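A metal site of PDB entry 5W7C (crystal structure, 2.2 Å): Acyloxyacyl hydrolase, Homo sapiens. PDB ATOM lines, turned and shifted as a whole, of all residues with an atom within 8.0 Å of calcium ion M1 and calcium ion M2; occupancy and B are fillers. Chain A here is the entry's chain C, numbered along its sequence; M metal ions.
The backbone carbonyl oxygen (O) of Val 61 binds calcium ion M2, at 2.3 Å.
OD2 of Asp 36 is bound to calcium ion M2.
Calcium ion M2 is bound by the side-chain carboxylate (OD2) of Asp 34 (2.3 Å).
O of Asn 55 binds calcium ion M2 (2.4 Å).
The side-chain carboxylate (OD2) of Asp 53 binds calcium ion M2 (2.5 Å).
Calcium ion M2 is bound by the backbone carbonyl oxygen (O) of Asp 58 (2.6 Å).
The side-chain carboxylate (OD1) of Asp 53 is bound to calcium ion M2.
The side-chain carboxylate (OD1) of Asp 34 is bound to calcium ion M1, 2.3 Å away.
Calcium ion M1 is bound by OD1 of Asp 36 (2.3 Å).
Calcium ion M1 is bound by the side-chain carboxylate (OD2) of Asp 53 (2.3 Å).
O of Tyr 38 binds calcium ion M1 (2.3 Å).
Calcium ion M1 is bound by the side-chain carboxylate (OD1) of Asp 32.
Calcium ion M1 is bound by OD1 of Asp 56 (2.5 Å).
Calcium ion M1 has six donor atoms within binding distance.
Of the 27 residues printed, 6 come within 4 Å of calcium ion M1.
The backbone NH (N) of Asp 53 lies within hydrogen-bond range of the backbone carbonyl oxygen (O) of Ser 39 (3.0 Å).
The backbone carbonyl oxygen (O) of Pro 63 sits at hydrogen-bond distance from the side-chain hydroxyl (OH) of Tyr 38, at 3.5 Å.
OD1 of Asp 32 sits close to N of Ser 35, at 3.3 Å.
N of Lys 37 sits at hydrogen-bond distance from OD2 of Asp 32, 2.7 Å away.
The side-chain amide nitrogen of Asn 55 lies within hydrogen-bond range of the side-chain amide oxygen of Gln 74 (2.7 Å).
OD2 of Asp 56 is in hydrogen-bond range of N of Val 33.
OD1 of Asp 58 sits at hydrogen-bond distance from N of Ser 60, at 2.9 Å.
The side-chain sulfur of Cys 54 forms a disulfide with the side-chain sulfur of Cys 78 (2.0 Å).
Six residues have an atom within 4 Å of calcium ion M2: Asp 34, Asp 36, Asp 53, Asn 55, Asp 58 and Val 61.
Along chain A the residues within 4 Å of calcium ion M2 span positions 34 to 61.
The nearest printed residue that does not touch calcium ion M2 is Asp 56 (4.1 Å).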
ATOM      1  N   PRO A  29       7.276  -3.747  22.193  1.00  0.00           N
ATOM      2  CA  PRO A  29       8.319  -4.736  22.471  1.00  0.00           C
ATOM      3  C   PRO A  29       8.364  -5.841  21.420  1.00  0.00           C
ATOM      4  O   PRO A  29       7.325  -6.340  20.980  1.00  0.00           O
ATOM      5  CB  PRO A  29       7.926  -5.287  23.847  1.00  0.00           C
ATOM      6  CG  PRO A  29       6.493  -4.898  24.044  1.00  0.00           C
ATOM      7  CD  PRO A  29       6.327  -3.611  23.302  1.00  0.00           C
ATOM      8  N   LYS A  31       9.855  -8.770  22.156  1.00  0.00           N
ATOM      9  CA  LYS A  31       9.582  -9.956  22.979  1.00  0.00           C
ATOM     10  C   LYS A  31       8.318  -9.676  23.785  1.00  0.00           C
ATOM     11  O   LYS A  31       8.359  -8.956  24.789  1.00  0.00           O
ATOM     12  CB  LYS A  31      10.779 -10.290  23.854  1.00  0.00           C
ATOM     13  CG  LYS A  31      11.789 -11.167  23.132  1.00  0.00           C
ATOM     14  CD  LYS A  31      13.094 -11.318  23.890  1.00  0.00           C
ATOM     15  CE  LYS A  31      14.108 -12.083  23.056  1.00  0.00           C
ATOM     16  NZ  LYS A  31      15.277 -12.541  23.868  1.00  0.00           N
ATOM     17  N   ASP A  32       7.204 -10.253  23.343  1.00  0.00           N
ATOM     18  CA  ASP A  32       5.888  -9.935  23.864  1.00  0.00           C
ATOM     19  C   ASP A  32       4.910 -11.021  23.440  1.00  0.00           C
ATOM     20  O   ASP A  32       4.156 -10.857  22.472  1.00  0.00           O
ATOM     21  CB  ASP A  32       5.432  -8.559  23.354  1.00  0.00           C
ATOM     22  CG  ASP A  32       4.160  -8.084  24.002  1.00  0.00           C
ATOM     23  OD1 ASP A  32       3.794  -8.612  25.073  1.00  0.00           O
ATOM     24  OD2 ASP A  32       3.514  -7.165  23.438  1.00  0.00           O
ATOM     25  N   VAL A  33       4.924 -12.149  24.148  1.00  0.00           N
ATOM     26  CA  VAL A  33       4.199 -13.334  23.700  1.00  0.00           C
ATOM     27  C   VAL A  33       2.694 -13.076  23.715  1.00  0.00           C
ATOM     28  O   VAL A  33       1.987 -13.382  22.743  1.00  0.00           O
ATOM     29  CB  VAL A  33       4.583 -14.553  24.559  1.00  0.00           C
ATOM     30  CG1 VAL A  33       3.742 -15.769  24.184  1.00  0.00           C
ATOM     31  CG2 VAL A  33       6.060 -14.859  24.392  1.00  0.00           C
ATOM     32  N   ASP A  34       2.182 -12.527  24.806  1.00  0.00           N
ATOM     33  CA  ASP A  34       0.745 -12.257  24.914  1.00  0.00           C
ATOM     34  C   ASP A  34       0.339 -10.960  24.232  1.00  0.00           C
ATOM     35  O   ASP A  34      -0.853 -10.635  24.212  1.00  0.00           O
ATOM     36  CB  ASP A  34       0.321 -12.236  26.384  1.00  0.00           C
ATOM     37  CG  ASP A  34       1.121 -11.249  27.214  1.00  0.00           C
ATOM     38  OD1 ASP A  34       1.683 -10.291  26.640  1.00  0.00           O
ATOM     39  OD2 ASP A  34       1.183 -11.432  28.446  1.00  0.00           O
ATOM     40  N   SER A  35       1.293 -10.196  23.686  1.00  0.00           N
ATOM     41  CA  SER A  35       0.982  -9.028  22.856  1.00  0.00           C
ATOM     42  C   SER A  35       0.210  -7.962  23.636  1.00  0.00           C
ATOM     43  O   SER A  35      -0.704  -7.332  23.115  1.00  0.00           O
ATOM     44  CB  SER A  35       0.223  -9.423  21.602  1.00  0.00           C
ATOM     45  OG  SER A  35       1.052 -10.107  20.674  1.00  0.00           O
ATOM     46  N   ASP A  36       0.589  -7.739  24.894  1.00  0.00           N
ATOM     47  CA  ASP A  36       0.025  -6.654  25.677  1.00  0.00           C
ATOM     48  C   ASP A  36       0.960  -5.459  25.770  1.00  0.00           C
ATOM     49  O   ASP A  36       0.683  -4.521  26.529  1.00  0.00           O
ATOM     50  CB  ASP A  36      -0.354  -7.132  27.089  1.00  0.00           C
ATOM     51  CG  ASP A  36       0.799  -7.750  27.838  1.00  0.00           C
ATOM     52  OD1 ASP A  36       1.963  -7.458  27.496  1.00  0.00           O
ATOM     53  OD2 ASP A  36       0.541  -8.523  28.781  1.00  0.00           O
ATOM     54  N   LYS A  37       2.056  -5.460  25.004  1.00  0.00           N
ATOM     55  CA  LYS A  37       3.009  -4.359  24.884  1.00  0.00           C
ATOM     56  C   LYS A  37       3.922  -4.248  26.088  1.00  0.00           C
ATOM     57  O   LYS A  37       4.660  -3.257  26.196  1.00  0.00           O
ATOM     58  CB  LYS A  37       2.305  -3.018  24.658  1.00  0.00           C
ATOM     59  CG  LYS A  37       1.330  -3.023  23.485  1.00  0.00           C
ATOM     60  CD  LYS A  37       0.841  -1.627  23.153  1.00  0.00           C
ATOM     61  CE  LYS A  37      -0.297  -1.651  22.151  1.00  0.00           C
ATOM     62  NZ  LYS A  37      -1.544  -1.078  22.746  1.00  0.00           N
ATOM     63  N   TYR A  38       3.922  -5.223  26.994  1.00  0.00           N
ATOM     64  CA  TYR A  38       4.888  -5.291  28.082  1.00  0.00           C
ATOM     65  C   TYR A  38       5.749  -6.543  27.896  1.00  0.00           C
ATOM     66  O   TYR A  38       5.247  -7.577  27.435  1.00  0.00           O
ATOM     67  CB  TYR A  38       4.197  -5.301  29.443  1.00  0.00           C
ATOM     68  CG  TYR A  38       3.446  -4.028  29.745  1.00  0.00           C
ATOM     69  CD1 TYR A  38       4.059  -2.987  30.428  1.00  0.00           C
ATOM     70  CD2 TYR A  38       2.139  -3.856  29.336  1.00  0.00           C
ATOM     71  CE1 TYR A  38       3.377  -1.810  30.702  1.00  0.00           C
ATOM     72  CE2 TYR A  38       1.450  -2.684  29.614  1.00  0.00           C
ATOM     73  CZ  TYR A  38       2.069  -1.672  30.293  1.00  0.00           C
ATOM     74  OH  TYR A  38       1.393  -0.501  30.572  1.00  0.00           O
ATOM     75  N   SER A  39       7.027  -6.435  28.245  1.00  0.00           N
ATOM     76  CA  SER A  39       8.008  -7.428  27.855  1.00  0.00           C
ATOM     77  C   SER A  39       8.743  -7.967  29.077  1.00  0.00           C
ATOM     78  O   SER A  39       8.741  -7.363  30.156  1.00  0.00           O
ATOM     79  CB  SER A  39       9.031  -6.830  26.870  1.00  0.00           C
ATOM     80  OG  SER A  39       9.994  -7.782  26.475  1.00  0.00           O
ATOM     81  N   VAL A  40       9.358  -9.144  28.893  1.00  0.00           N
ATOM     82  CA  VAL A  40      10.274  -9.709  29.880  1.00  0.00           C
ATOM     83  C   VAL A  40      11.724  -9.397  29.546  1.00  0.00           C
ATOM     84  O   VAL A  40      12.603  -9.587  30.396  1.00  0.00           O
ATOM     85  CB  VAL A  40      10.089 -11.241  30.000  1.00  0.00           C
ATOM     86  CG1 VAL A  40       8.665 -11.575  30.423  1.00  0.00           C
ATOM     87  CG2 VAL A  40      10.453 -11.939  28.696  1.00  0.00           C
ATOM     88  N   GLY A  51       6.950  -1.094  32.361  1.00  0.00           N
ATOM     89  CA  GLY A  51       7.016  -2.065  33.439  1.00  0.00           C
ATOM     90  C   GLY A  51       7.215  -3.473  32.909  1.00  0.00           C
ATOM     91  O   GLY A  51       6.646  -3.860  31.882  1.00  0.00           O
ATOM     92  N   ARG A  52       8.031  -4.241  33.614  1.00  0.00           N
ATOM     93  CA  ARG A  52       8.279  -5.632  33.234  1.00  0.00           C
ATOM     94  C   ARG A  52       6.991  -6.439  33.360  1.00  0.00           C
ATOM     95  O   ARG A  52       6.279  -6.353  34.363  1.00  0.00           O
ATOM     96  CB  ARG A  52       9.368  -6.222  34.129  1.00  0.00           C
ATOM     97  CG  ARG A  52       9.870  -7.590  33.716  1.00  0.00           C
ATOM     98  CD  ARG A  52      10.807  -8.141  34.779  1.00  0.00           C
ATOM     99  NE  ARG A  52      11.756  -9.117  34.242  1.00  0.00           N
ATOM    100  CZ  ARG A  52      13.085  -8.998  34.260  1.00  0.00           C
ATOM    101  NH1 ARG A  52      13.664  -7.935  34.804  1.00  0.00           N
ATOM    102  NH2 ARG A  52      13.834  -9.959  33.734  1.00  0.00           N
ATOM    103  N   ASP A  53       6.694  -7.215  32.327  1.00  0.00           N
ATOM    104  CA  ASP A  53       5.515  -8.077  32.340  1.00  0.00           C
ATOM    105  C   ASP A  53       5.743  -9.244  33.285  1.00  0.00           C
ATOM    106  O   ASP A  53       6.636 -10.069  33.065  1.00  0.00           O
ATOM    107  CB  ASP A  53       5.210  -8.584  30.929  1.00  0.00           C
ATOM    108  CG  ASP A  53       3.819  -9.171  30.801  1.00  0.00           C
ATOM    109  OD1 ASP A  53       3.133  -9.359  31.835  1.00  0.00           O
ATOM    110  OD2 ASP A  53       3.403  -9.459  29.657  1.00  0.00           O
ATOM    111  N   CYS A  54       4.943  -9.317  34.366  1.00  0.00           N
ATOM    112  CA  CYS A  54       5.082 -10.411  35.314  1.00  0.00           C
ATOM    113  C   CYS A  54       4.516 -11.723  34.783  1.00  0.00           C
ATOM    114  O   CYS A  54       4.820 -12.775  35.352  1.00  0.00           O
ATOM    115  CB  CYS A  54       4.392 -10.044  36.637  1.00  0.00           C
ATOM    116  SG  CYS A  54       2.680  -9.459  36.486  1.00  0.00           S
ATOM    117  N   ASN A  55       3.709 -11.682  33.725  1.00  0.00           N
ATOM    118  CA  ASN A  55       3.201 -12.908  33.104  1.00  0.00           C
ATOM    119  C   ASN A  55       3.059 -12.634  31.610  1.00  0.00           C
ATOM    120  O   ASN A  55       2.024 -12.144  31.151  1.00  0.00           O
ATOM    121  CB  ASN A  55       1.879 -13.355  33.709  1.00  0.00           C
ATOM    122  CG  ASN A  55       1.555 -14.800  33.384  1.00  0.00           C
ATOM    123  OD1 ASN A  55       1.958 -15.298  32.335  1.00  0.00           O
ATOM    124  ND2 ASN A  55       0.831 -15.473  34.273  1.00  0.00           N
ATOM    125  N   ASP A  56       4.093 -12.985  30.847  1.00  0.00           N
ATOM    126  CA  ASP A  56       4.084 -12.777  29.408  1.00  0.00           C
ATOM    127  C   ASP A  56       3.202 -13.774  28.676  1.00  0.00           C
ATOM    128  O   ASP A  56       3.175 -13.755  27.437  1.00  0.00           O
ATOM    129  CB  ASP A  56       5.517 -12.840  28.855  1.00  0.00           C
ATOM    130  CG  ASP A  56       5.644 -12.200  27.484  1.00  0.00           C
ATOM    131  OD1 ASP A  56       4.948 -11.206  27.216  1.00  0.00           O
ATOM    132  OD2 ASP A  56       6.448 -12.712  26.669  1.00  0.00           O
ATOM    133  N   SER A  57       2.494 -14.641  29.395  1.00  0.00           N
ATOM    134  CA  SER A  57       1.542 -15.574  28.795  1.00  0.00           C
ATOM    135  C   SER A  57       0.103 -15.276  29.200  1.00  0.00           C
ATOM    136  O   SER A  57      -0.743 -16.170  29.151  1.00  0.00           O
ATOM    137  CB  SER A  57       1.911 -17.012  29.171  1.00  0.00           C
ATOM    138  OG  SER A  57       3.212 -17.343  28.718  1.00  0.00           O
ATOM    139  N   ASP A  58      -0.177 -14.041  29.611  1.00  0.00           N
ATOM    140  CA  ASP A  58      -1.530 -13.648  29.981  1.00  0.00           C
ATOM    141  C   ASP A  58      -1.704 -12.173  29.607  1.00  0.00           C
ATOM    142  O   ASP A  58      -1.202 -11.290  30.316  1.00  0.00           O
ATOM    143  CB  ASP A  58      -1.783 -13.879  31.465  1.00  0.00           C
ATOM    144  CG  ASP A  58      -3.257 -13.752  31.838  1.00  0.00           C
ATOM    145  OD1 ASP A  58      -3.995 -13.079  31.095  1.00  0.00           O
ATOM    146  OD2 ASP A  58      -3.664 -14.335  32.871  1.00  0.00           O
ATOM    147  N   GLU A  59      -2.404 -11.927  28.503  1.00  0.00           N
ATOM    148  CA  GLU A  59      -2.655 -10.563  28.064  1.00  0.00           C
ATOM    149  C   GLU A  59      -3.431  -9.752  29.090  1.00  0.00           C
ATOM    150  O   GLU A  59      -3.399  -8.526  29.046  1.00  0.00           O
ATOM    151  CB  GLU A  59      -3.421 -10.569  26.739  1.00  0.00           C
ATOM    152  CG  GLU A  59      -4.850 -11.069  26.863  1.00  0.00           C
ATOM    153  CD  GLU A  59      -5.519 -11.298  25.515  1.00  0.00           C
ATOM    154  OE1 GLU A  59      -5.267 -10.491  24.584  1.00  0.00           O
ATOM    155  OE2 GLU A  59      -6.280 -12.270  25.380  1.00  0.00           O
ATOM    156  N   SER A  60      -4.136 -10.421  30.002  1.00  0.00           N
ATOM    157  CA  SER A  60      -4.886  -9.744  31.049  1.00  0.00           C
ATOM    158  C   SER A  60      -4.042  -9.433  32.270  1.00  0.00           C
ATOM    159  O   SER A  60      -4.580  -8.980  33.291  1.00  0.00           O
ATOM    160  CB  SER A  60      -6.093 -10.591  31.462  1.00  0.00           C
ATOM    161  OG  SER A  60      -6.980 -10.787  30.366  1.00  0.00           O
ATOM    162  N   VAL A  61      -2.728  -9.652  32.202  1.00  0.00           N
ATOM    163  CA  VAL A  61      -1.807  -9.365  33.287  1.00  0.00           C
ATOM    164  C   VAL A  61      -0.732  -8.434  32.758  1.00  0.00           C
ATOM    165  O   VAL A  61       0.019  -8.801  31.840  1.00  0.00           O
ATOM    166  CB  VAL A  61      -1.182 -10.647  33.867  1.00  0.00           C
ATOM    167  CG1 VAL A  61      -0.166 -10.312  34.951  1.00  0.00           C
ATOM    168  CG2 VAL A  61      -2.273 -11.560  34.419  1.00  0.00           C
ATOM    169  N   TYR A  62      -0.639  -7.237  33.320  1.00  0.00           N
ATOM    170  CA  TYR A  62       0.347  -6.258  32.909  1.00  0.00           C
ATOM    171  C   TYR A  62       0.306  -5.089  33.892  1.00  0.00           C
ATOM    172  O   TYR A  62      -0.695  -4.912  34.593  1.00  0.00           O
ATOM    173  CB  TYR A  62       0.081  -5.754  31.480  1.00  0.00           C
ATOM    174  CG  TYR A  62      -1.335  -5.274  31.241  1.00  0.00           C
ATOM    175  CD1 TYR A  62      -1.721  -3.992  31.600  1.00  0.00           C
ATOM    176  CD2 TYR A  62      -2.284  -6.105  30.669  1.00  0.00           C
ATOM    177  CE1 TYR A  62      -3.008  -3.548  31.396  1.00  0.00           C
ATOM    178  CE2 TYR A  62      -3.569  -5.672  30.448  1.00  0.00           C
ATOM    179  CZ  TYR A  62      -3.935  -4.396  30.813  1.00  0.00           C
ATOM    180  OH  TYR A  62      -5.220  -3.964  30.592  1.00  0.00           O
ATOM    181  N   PRO A  63       1.367  -4.292  33.950  1.00  0.00           N
ATOM    182  CA  PRO A  63       1.370  -3.134  34.859  1.00  0.00           C
ATOM    183  C   PRO A  63       0.244  -2.164  34.539  1.00  0.00           C
ATOM    184  O   PRO A  63      -0.093  -1.934  33.376  1.00  0.00           O
ATOM    185  CB  PRO A  63       2.745  -2.508  34.633  1.00  0.00           C
ATOM    186  CG  PRO A  63       3.593  -3.613  34.103  1.00  0.00           C
ATOM    187  CD  PRO A  63       2.676  -4.474  33.299  1.00  0.00           C
ATOM    188  N   GLN A  74      -3.406 -14.471  41.466  1.00  0.00           N
ATOM    189  CA  GLN A  74      -2.358 -13.976  40.589  1.00  0.00           C
ATOM    190  C   GLN A  74      -2.176 -12.481  40.810  1.00  0.00           C
ATOM    191  O   GLN A  74      -3.144 -11.757  41.081  1.00  0.00           O
ATOM    192  CB  GLN A  74      -2.673 -14.249  39.116  1.00  0.00           C
ATOM    193  CG  GLN A  74      -1.683 -15.171  38.424  1.00  0.00           C
ATOM    194  CD  GLN A  74      -1.548 -14.900  36.940  1.00  0.00           C
ATOM    195  OE1 GLN A  74      -0.486 -14.524  36.461  1.00  0.00           O
ATOM    196  NE2 GLN A  74      -2.638 -15.095  36.204  1.00  0.00           N
ATOM    197  N   SER A  76      -2.119  -9.540  39.079  1.00  0.00           N
ATOM    198  CA  SER A  76      -2.595  -9.172  37.751  1.00  0.00           C
ATOM    199  C   SER A  76      -2.044  -7.846  37.253  1.00  0.00           C
ATOM    200  O   SER A  76      -2.188  -7.544  36.055  1.00  0.00           O
ATOM    201  CB  SER A  76      -4.129  -9.126  37.738  1.00  0.00           C
ATOM    202  OG  SER A  76      -4.615  -8.045  38.517  1.00  0.00           O
ATOM    203  N   CYS A  78       1.302  -6.762  38.232  1.00  0.00           N
ATOM    204  CA  CYS A  78       2.766  -6.824  38.299  1.00  0.00           C
ATOM    205  C   CYS A  78       3.350  -5.871  39.330  1.00  0.00           C
ATOM    206  O   CYS A  78       4.539  -5.522  39.242  1.00  0.00           O
ATOM    207  CB  CYS A  78       3.381  -6.526  36.930  1.00  0.00           C
ATOM    208  SG  CYS A  78       2.822  -7.629  35.603  1.00  0.00           S
HETATM  209 CA    CA M   1       3.515  -9.150  27.358  1.00  0.00          CA
HETATM  210 CA    CA M   2       1.102 -10.091  30.326  1.00  0.00          CA
